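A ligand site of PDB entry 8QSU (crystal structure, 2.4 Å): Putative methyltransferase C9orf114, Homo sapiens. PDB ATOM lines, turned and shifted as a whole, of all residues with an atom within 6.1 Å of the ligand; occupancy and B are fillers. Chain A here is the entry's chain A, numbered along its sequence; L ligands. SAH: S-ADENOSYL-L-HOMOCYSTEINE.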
ATOM      1  N   ILE A  14       3.164  11.782  26.154  1.00  0.00           N
ATOM      2  CA  ILE A  14       3.351  12.134  24.745  1.00  0.00           C
ATOM      3  C   ILE A  14       4.592  12.999  24.545  1.00  0.00           C
ATOM      4  O   ILE A  14       5.290  12.856  23.540  1.00  0.00           O
ATOM      5  CB  ILE A  14       2.077  12.845  24.245  1.00  0.00           C
ATOM      6  CG1 ILE A  14       0.965  11.824  24.086  1.00  0.00           C
ATOM      7  CG2 ILE A  14       2.271  13.469  22.939  1.00  0.00           C
ATOM      8  CD1 ILE A  14       1.462  10.576  23.442  1.00  0.00           C
ATOM      9  N   GLY A 219     -13.472   5.850  23.432  1.00  0.00           N
ATOM     10  CA  GLY A 219     -12.068   5.479  23.431  1.00  0.00           C
ATOM     11  C   GLY A 219     -11.582   5.215  22.020  1.00  0.00           C
ATOM     12  O   GLY A 219     -12.334   4.769  21.157  1.00  0.00           O
ATOM     13  N   THR A 220     -10.310   5.502  21.785  1.00  0.00           N
ATOM     14  CA  THR A 220      -9.713   5.411  20.464  1.00  0.00           C
ATOM     15  C   THR A 220      -8.621   4.354  20.467  1.00  0.00           C
ATOM     16  O   THR A 220      -7.722   4.378  21.306  1.00  0.00           O
ATOM     17  CB  THR A 220      -9.137   6.741  20.033  1.00  0.00           C
ATOM     18  OG1 THR A 220      -8.239   7.217  21.050  1.00  0.00           O
ATOM     19  CG2 THR A 220     -10.258   7.749  19.834  1.00  0.00           C
ATOM     20  N   SER A 221      -8.696   3.434  19.511  1.00  0.00           N
ATOM     21  CA  SER A 221      -7.654   2.436  19.326  1.00  0.00           C
ATOM     22  C   SER A 221      -7.751   1.878  17.918  1.00  0.00           C
ATOM     23  O   SER A 221      -8.792   1.963  17.261  1.00  0.00           O
ATOM     24  CB  SER A 221      -7.759   1.347  20.389  1.00  0.00           C
ATOM     25  OG  SER A 221      -6.944   0.239  20.097  1.00  0.00           O
ATOM     26  N   GLU A 222      -6.652   1.294  17.448  1.00  0.00           N
ATOM     27  CA  GLU A 222      -6.707   0.578  16.177  1.00  0.00           C
ATOM     28  C   GLU A 222      -7.401  -0.767  16.328  1.00  0.00           C
ATOM     29  O   GLU A 222      -7.676  -1.422  15.312  1.00  0.00           O
ATOM     30  CB  GLU A 222      -5.291   0.385  15.591  1.00  0.00           C
ATOM     31  CG  GLU A 222      -4.422  -0.625  16.337  1.00  0.00           C
ATOM     32  CD  GLU A 222      -2.926  -0.357  16.189  1.00  0.00           C
ATOM     33  OE1 GLU A 222      -2.222  -1.212  15.597  1.00  0.00           O
ATOM     34  OE2 GLU A 222      -2.455   0.702  16.655  1.00  0.00           O
ATOM     35  N   ARG A 223      -7.707  -1.175  17.555  1.00  0.00           N
ATOM     36  CA  ARG A 223      -8.445  -2.397  17.831  1.00  0.00           C
ATOM     37  C   ARG A 223      -9.920  -2.156  18.117  1.00  0.00           C
ATOM     38  O   ARG A 223     -10.650  -3.106  18.407  1.00  0.00           O
ATOM     39  CB  ARG A 223      -7.817  -3.142  19.008  1.00  0.00           C
ATOM     40  CG  ARG A 223      -6.470  -3.749  18.712  1.00  0.00           C
ATOM     41  CD  ARG A 223      -5.823  -4.204  20.002  1.00  0.00           C
ATOM     42  NE  ARG A 223      -4.681  -3.369  20.346  1.00  0.00           N
ATOM     43  CZ  ARG A 223      -3.420  -3.767  20.257  1.00  0.00           C
ATOM     44  NH1 ARG A 223      -3.112  -5.008  19.906  1.00  0.00           N
ATOM     45  NH2 ARG A 223      -2.443  -2.905  20.523  1.00  0.00           N
ATOM     46  N   VAL A 241     -11.138   9.934  24.412  1.00  0.00           N
ATOM     47  CA  VAL A 241      -9.916   9.627  25.142  1.00  0.00           C
ATOM     48  C   VAL A 241      -8.892   8.980  24.212  1.00  0.00           C
ATOM     49  O   VAL A 241      -9.203   8.030  23.487  1.00  0.00           O
ATOM     50  CB  VAL A 241     -10.179   8.699  26.334  1.00  0.00           C
ATOM     51  CG1 VAL A 241      -8.913   8.580  27.181  1.00  0.00           C
ATOM     52  CG2 VAL A 241     -11.356   9.210  27.159  1.00  0.00           C
ATOM     53  N   PHE A 242      -7.646   9.463  24.308  1.00  0.00           N
ATOM     54  CA  PHE A 242      -6.538   9.083  23.442  1.00  0.00           C
ATOM     55  C   PHE A 242      -5.408   8.538  24.306  1.00  0.00           C
ATOM     56  O   PHE A 242      -5.139   9.072  25.386  1.00  0.00           O
ATOM     57  CB  PHE A 242      -6.034  10.275  22.638  1.00  0.00           C
ATOM     58  CG  PHE A 242      -7.067  10.841  21.705  1.00  0.00           C
ATOM     59  CD1 PHE A 242      -7.203  10.338  20.411  1.00  0.00           C
ATOM     60  CD2 PHE A 242      -7.897  11.879  22.111  1.00  0.00           C
ATOM     61  CE1 PHE A 242      -8.159  10.860  19.541  1.00  0.00           C
ATOM     62  CE2 PHE A 242      -8.845  12.398  21.256  1.00  0.00           C
ATOM     63  CZ  PHE A 242      -8.995  11.887  19.981  1.00  0.00           C
ATOM     64  N   GLY A 243      -4.742   7.487  23.833  1.00  0.00           N
ATOM     65  CA  GLY A 243      -3.620   6.926  24.543  1.00  0.00           C
ATOM     66  C   GLY A 243      -2.309   7.536  24.088  1.00  0.00           C
ATOM     67  O   GLY A 243      -2.251   8.490  23.310  1.00  0.00           O
ATOM     68  N   GLY A 244      -1.220   6.969  24.601  1.00  0.00           N
ATOM     69  CA  GLY A 244       0.098   7.437  24.232  1.00  0.00           C
ATOM     70  C   GLY A 244       0.815   6.461  23.338  1.00  0.00           C
ATOM     71  O   GLY A 244       0.188   5.721  22.570  1.00  0.00           O
ATOM     72  N   LEU A 245       2.138   6.464  23.422  1.00  0.00           N
ATOM     73  CA  LEU A 245       2.949   5.535  22.648  1.00  0.00           C
ATOM     74  C   LEU A 245       2.461   4.094  22.813  1.00  0.00           C
ATOM     75  O   LEU A 245       2.330   3.348  21.831  1.00  0.00           O
ATOM     76  CB  LEU A 245       4.403   5.664  23.063  1.00  0.00           C
ATOM     77  CG  LEU A 245       5.382   4.730  22.363  1.00  0.00           C
ATOM     78  CD1 LEU A 245       5.193   4.860  20.859  1.00  0.00           C
ATOM     79  CD2 LEU A 245       6.813   5.049  22.772  1.00  0.00           C
ATOM     80  N   GLN A 246       2.164   3.690  24.042  1.00  0.00           N
ATOM     81  CA  GLN A 246       1.752   2.325  24.356  1.00  0.00           C
ATOM     82  C   GLN A 246       0.232   2.117  24.302  1.00  0.00           C
ATOM     83  O   GLN A 246      -0.252   1.067  24.710  1.00  0.00           O
ATOM     84  CB  GLN A 246       2.262   1.931  25.754  1.00  0.00           C
ATOM     85  CG  GLN A 246       3.687   2.340  26.058  1.00  0.00           C
ATOM     86  CD  GLN A 246       4.710   1.399  25.453  1.00  0.00           C
ATOM     87  OE1 GLN A 246       4.362   0.418  24.789  1.00  0.00           O
ATOM     88  NE2 GLN A 246       5.988   1.691  25.692  1.00  0.00           N
ATOM     89  N   GLY A 247      -0.517   3.110  23.836  1.00  0.00           N
ATOM     90  CA  GLY A 247      -1.954   2.984  23.767  1.00  0.00           C
ATOM     91  C   GLY A 247      -2.629   3.137  25.130  1.00  0.00           C
ATOM     92  O   GLY A 247      -1.989   3.279  26.170  1.00  0.00           O
ATOM     93  N   LEU A 248      -3.965   3.105  25.093  1.00  0.00           N
ATOM     94  CA  LEU A 248      -4.738   3.210  26.313  1.00  0.00           C
ATOM     95  C   LEU A 248      -4.537   2.014  27.231  1.00  0.00           C
ATOM     96  O   LEU A 248      -4.921   2.073  28.407  1.00  0.00           O
ATOM     97  CB  LEU A 248      -6.235   3.354  25.980  1.00  0.00           C
ATOM     98  CG  LEU A 248      -6.715   4.721  25.473  1.00  0.00           C
ATOM     99  CD1 LEU A 248      -8.167   4.644  25.021  1.00  0.00           C
ATOM    100  CD2 LEU A 248      -6.547   5.786  26.543  1.00  0.00           C
ATOM    101  N   GLU A 249      -3.923   0.935  26.748  1.00  0.00           N
ATOM    102  CA  GLU A 249      -3.711  -0.234  27.585  1.00  0.00           C
ATOM    103  C   GLU A 249      -2.763   0.065  28.738  1.00  0.00           C
ATOM    104  O   GLU A 249      -2.817  -0.602  29.777  1.00  0.00           O
ATOM    105  CB  GLU A 249      -3.183  -1.401  26.754  1.00  0.00           C
ATOM    106  CG  GLU A 249      -4.233  -2.112  25.890  1.00  0.00           C
ATOM    107  CD  GLU A 249      -4.612  -1.342  24.609  1.00  0.00           C
ATOM    108  OE1 GLU A 249      -4.273  -0.138  24.502  1.00  0.00           O
ATOM    109  OE2 GLU A 249      -5.242  -1.954  23.716  1.00  0.00           O
ATOM    110  N   VAL A 271     -13.540   2.926  19.269  1.00  0.00           N
ATOM    111  CA  VAL A 271     -13.559   3.064  17.814  1.00  0.00           C
ATOM    112  C   VAL A 271     -12.148   3.174  17.249  1.00  0.00           C
ATOM    113  O   VAL A 271     -11.277   3.837  17.819  1.00  0.00           O
ATOM    114  CB  VAL A 271     -14.405   4.270  17.340  1.00  0.00           C
ATOM    115  CG1 VAL A 271     -15.861   4.027  17.672  1.00  0.00           C
ATOM    116  CG2 VAL A 271     -13.909   5.556  17.982  1.00  0.00           C
ATOM    117  N   ASN A 272     -11.939   2.457  16.141  1.00  0.00           N
ATOM    118  CA  ASN A 272     -10.884   2.735  15.158  1.00  0.00           C
ATOM    119  C   ASN A 272     -11.436   3.744  14.164  1.00  0.00           C
ATOM    120  O   ASN A 272     -12.431   3.479  13.481  1.00  0.00           O
ATOM    121  CB  ASN A 272     -10.484   1.431  14.462  1.00  0.00           C
ATOM    122  CG  ASN A 272      -9.344   1.602  13.429  1.00  0.00           C
ATOM    123  OD1 ASN A 272      -9.179   2.663  12.803  1.00  0.00           O
ATOM    124  ND2 ASN A 272      -8.566   0.539  13.254  1.00  0.00           N
ATOM    125  N   THR A 273     -10.810   4.915  14.093  1.00  0.00           N
ATOM    126  CA  THR A 273     -11.271   5.982  13.216  1.00  0.00           C
ATOM    127  C   THR A 273     -10.450   6.146  11.948  1.00  0.00           C
ATOM    128  O   THR A 273     -10.538   7.198  11.299  1.00  0.00           O
ATOM    129  CB  THR A 273     -11.300   7.313  13.962  1.00  0.00           C
ATOM    130  OG1 THR A 273      -9.954   7.746  14.208  1.00  0.00           O
ATOM    131  CG2 THR A 273     -12.035   7.170  15.255  1.00  0.00           C
ATOM    132  N   CYS A 274      -9.633   5.158  11.567  1.00  0.00           N
ATOM    133  CA  CYS A 274      -8.923   5.179  10.289  1.00  0.00           C
ATOM    134  C   CYS A 274      -8.860   3.746   9.804  1.00  0.00           C
ATOM    135  O   CYS A 274      -7.904   3.012  10.085  1.00  0.00           O
ATOM    136  CB  CYS A 274      -7.518   5.779  10.411  1.00  0.00           C
ATOM    137  SG  CYS A 274      -6.807   6.686   8.915  1.00  0.00           S
ATOM    138  N   PRO A 275      -9.877   3.310   9.062  1.00  0.00           N
ATOM    139  CA  PRO A 275      -9.822   1.977   8.469  1.00  0.00           C
ATOM    140  C   PRO A 275      -8.662   1.906   7.480  1.00  0.00           C
ATOM    141  O   PRO A 275      -8.412   2.854   6.729  1.00  0.00           O
ATOM    142  CB  PRO A 275     -11.178   1.844   7.771  1.00  0.00           C
ATOM    143  CG  PRO A 275     -11.842   3.196   7.818  1.00  0.00           C
ATOM    144  CD  PRO A 275     -10.866   4.174   8.391  1.00  0.00           C
ATOM    145  N   GLN A 277      -5.313   1.992   7.782  1.00  0.00           N
ATOM    146  CA  GLN A 277      -4.214   2.947   7.834  1.00  0.00           C
ATOM    147  C   GLN A 277      -3.012   2.433   7.041  1.00  0.00           C
ATOM    148  O   GLN A 277      -2.779   1.222   6.940  1.00  0.00           O
ATOM    149  CB  GLN A 277      -3.834   3.234   9.290  1.00  0.00           C
ATOM    150  CG  GLN A 277      -3.764   2.001  10.172  1.00  0.00           C
ATOM    151  CD  GLN A 277      -3.446   2.353  11.608  1.00  0.00           C
ATOM    152  OE1 GLN A 277      -4.330   2.470  12.442  1.00  0.00           O
ATOM    153  NE2 GLN A 277      -2.154   2.504  11.903  1.00  0.00           N
ATOM    154  N   THR A 281       1.476   3.023  12.835  1.00  0.00           N
ATOM    155  CA  THR A 281       1.073   3.756  14.034  1.00  0.00           C
ATOM    156  C   THR A 281       0.662   5.169  13.660  1.00  0.00           C
ATOM    157  O   THR A 281       1.331   5.836  12.866  1.00  0.00           O
ATOM    158  CB  THR A 281       2.220   3.813  15.052  1.00  0.00           C
ATOM    159  OG1 THR A 281       3.429   4.194  14.382  1.00  0.00           O
ATOM    160  CG2 THR A 281       2.410   2.450  15.739  1.00  0.00           C
ATOM    161  N   ILE A 282      -0.442   5.613  14.256  1.00  0.00           N
ATOM    162  CA  ILE A 282      -0.877   7.000  14.178  1.00  0.00           C
ATOM    163  C   ILE A 282      -0.518   7.659  15.498  1.00  0.00           C
ATOM    164  O   ILE A 282      -0.995   7.241  16.555  1.00  0.00           O
ATOM    165  CB  ILE A 282      -2.381   7.103  13.887  1.00  0.00           C
ATOM    166  CG1 ILE A 282      -2.739   6.318  12.614  1.00  0.00           C
ATOM    167  CG2 ILE A 282      -2.801   8.549  13.754  1.00  0.00           C
ATOM    168  CD1 ILE A 282      -4.237   6.216  12.329  1.00  0.00           C
ATOM    169  N   ARG A 283       0.325   8.672  15.441  1.00  0.00           N
ATOM    170  CA  ARG A 283       0.687   9.368  16.653  1.00  0.00           C
ATOM    171  C   ARG A 283      -0.507  10.117  17.217  1.00  0.00           C
ATOM    172  O   ARG A 283      -1.475  10.440  16.498  1.00  0.00           O
ATOM    173  CB  ARG A 283       1.854  10.307  16.382  1.00  0.00           C
ATOM    174  CG  ARG A 283       2.959   9.622  15.613  1.00  0.00           C
ATOM    175  CD  ARG A 283       3.866  10.640  14.972  1.00  0.00           C
ATOM    176  NE  ARG A 283       4.368  11.557  15.973  1.00  0.00           N
ATOM    177  CZ  ARG A 283       5.442  11.316  16.719  1.00  0.00           C
ATOM    178  NH1 ARG A 283       6.146  10.214  16.550  1.00  0.00           N
ATOM    179  NH2 ARG A 283       5.810  12.203  17.647  1.00  0.00           N
ATOM    180  N   THR A 284      -0.426  10.401  18.521  1.00  0.00           N
ATOM    181  CA  THR A 284      -1.554  10.959  19.262  1.00  0.00           C
ATOM    182  C   THR A 284      -2.011  12.273  18.658  1.00  0.00           C
ATOM    183  O   THR A 284      -3.214  12.502  18.463  1.00  0.00           O
ATOM    184  CB  THR A 284      -1.177  11.169  20.750  1.00  0.00           C
ATOM    185  OG1 THR A 284      -0.789   9.925  21.354  1.00  0.00           O
ATOM    186  CG2 THR A 284      -2.344  11.759  21.513  1.00  0.00           C
ATOM    187  N   ALA A 287      -3.730  11.373  15.633  1.00  0.00           N
ATOM    188  CA  ALA A 287      -4.979  10.675  15.927  1.00  0.00           C
ATOM    189  C   ALA A 287      -6.088  11.638  16.330  1.00  0.00           C
ATOM    190  O   ALA A 287      -7.246  11.416  15.960  1.00  0.00           O
ATOM    191  CB  ALA A 287      -4.729   9.626  16.998  1.00  0.00           C
ATOM    192  N   SER A 291      -9.521  11.722  14.527  1.00  0.00           N
ATOM    193  CA  SER A 291     -10.649  11.182  15.272  1.00  0.00           C
ATOM    194  C   SER A 291     -11.754  12.209  15.405  1.00  0.00           C
ATOM    195  O   SER A 291     -12.927  11.894  15.177  1.00  0.00           O
ATOM    196  CB  SER A 291     -10.173  10.714  16.646  1.00  0.00           C
ATOM    197  OG  SER A 291      -9.439   9.516  16.493  1.00  0.00           O
HETATM  198  N   SAH L   1       1.041   0.721  19.706  1.00  0.00           N
HETATM  199  CA  SAH L   1      -0.090   1.430  20.293  1.00  0.00           C
HETATM  200  CB  SAH L   1      -0.561   2.555  19.374  1.00  0.00           C
HETATM  201  CG  SAH L   1      -0.237   3.956  19.887  1.00  0.00           C
HETATM  202  SD  SAH L   1      -0.891   5.231  18.793  1.00  0.00           S
HETATM  203  C   SAH L   1      -1.242   0.460  20.590  1.00  0.00           C
HETATM  204  O   SAH L   1      -1.274  -0.671  20.095  1.00  0.00           O
HETATM  205  OXT SAH L   1      -2.183   0.785  21.312  1.00  0.00           O
HETATM  206  C5' SAH L   1      -1.315   6.460  20.063  1.00  0.00           C
HETATM  207  C4' SAH L   1      -2.813   6.734  20.222  1.00  0.00           C
HETATM  208  O4' SAH L   1      -3.424   7.226  19.034  1.00  0.00           O
HETATM  209  C3' SAH L   1      -3.606   5.495  20.604  1.00  0.00           C
HETATM  210  O3' SAH L   1      -3.576   5.281  21.997  1.00  0.00           O
HETATM  211  C2' SAH L   1      -5.002   5.805  20.118  1.00  0.00           C
HETATM  212  O2' SAH L   1      -5.701   6.537  21.110  1.00  0.00           O
HETATM  213  C1' SAH L   1      -4.737   6.706  18.913  1.00  0.00           C
HETATM  214  N9  SAH L   1      -4.888   5.914  17.651  1.00  0.00           N
HETATM  215  C8  SAH L   1      -3.906   5.314  16.901  1.00  0.00           C
HETATM  216  N7  SAH L   1      -4.483   4.683  15.834  1.00  0.00           N
HETATM  217  C5  SAH L   1      -5.818   4.876  15.900  1.00  0.00           C
HETATM  218  C6  SAH L   1      -6.888   4.473  15.107  1.00  0.00           C
HETATM  219  N6  SAH L   1      -6.699   3.737  14.019  1.00  0.00           N
HETATM  220  N1  SAH L   1      -8.185   4.833  15.469  1.00  0.00           N
HETATM  221  C2  SAH L   1      -8.413   5.594  16.590  1.00  0.00           C
HETATM  222  N3  SAH L   1      -7.352   5.994  17.381  1.00  0.00           N
HETATM  223  C4  SAH L   1      -6.086   5.644  17.038  1.00  0.00           C
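OG of Ser 221 sits at hydrogen-bond distance from N of Arg 223 (3.0 Å). The guanidinium group (NE) of Arg 223 is in salt-bridge range of the side-chain carboxylate (OE2) of Glu 249. The side-chain hydroxyl (OG1) of Thr 220 sits at hydrogen-bond distance from the backbone carbonyl oxygen (O) of Val 241 (2.7 Å). The backbone NH (N) of Asn 272 sits close to the backbone carbonyl oxygen (O) of Ser 221 (3.4 Å). OG1 of Thr 273 is in hydrogen-bond range of OG of Ser 291. The backbone carbonyl oxygen (O) of Ala 287 sits at hydrogen-bond distance from the side-chain hydroxyl (OG) of Ser 291 (3.0 Å). The backbone NH (N) of Ser 221 sits at hydrogen-bond distance from the backbone carbonyl oxygen (O) of Val 271, 3.1 Å away. The backbone NH of Val 271 sits at hydrogen-bond distance from the backbone carbonyl oxygen of Gly 219 (2.9 Å).
The guanidinium group of Arg 223 lies within salt-bridge range of an oxygen (O) of the ligand, at 2.6 Å. O2' of the ligand is in hydrogen-bond range of O of Thr 220 (3.0 Å). OG1 of Thr 220 sits at hydrogen-bond distance from O2' of the ligand (2.6 Å). The side-chain amide oxygen (OD1) of Asn 272 lies within hydrogen-bond range of a nitrogen (N6) of the ligand, at 3.0 Å. A nitrogen (N1) of the ligand lies within hydrogen-bond range of the backbone NH (N) of Thr 273, 3.0 Å away. An oxygen (O2') of the ligand is in hydrogen-bond range of the backbone NH (N) of Gly 243. OE1 of Gln 277 is in hydrogen-bond range of N6 of the ligand, 3.1 Å away.
O of Ser 221 lies close to N1 of the ligand, at 3.4 Å. O of Ile 282 lies close to SD of the ligand (3.0 Å). Merely in contact with the ligand: Glu 222 (3.8 Å), Phe 242 (3.6 Å), Gly 244 (3.0 Å), Leu 245 (3.3 Å), Gln 246 (3.9 Å), Gly 247 (3.3 Å), Leu 248 (3.8 Å), Glu 249 (3.9 Å), Val 271 (3.6 Å), Thr 284 (3.7 Å) and Ala 287 (3.4 Å). Hydrophobic or aromatic side chains within 4 Å of the ligand: Ile 282 and Ala 287. Of the 27 residues printed, 19 come within 4 Å of the ligand. The nearest printed residue that does not touch the ligand is Ser 291 (4.1 Å).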
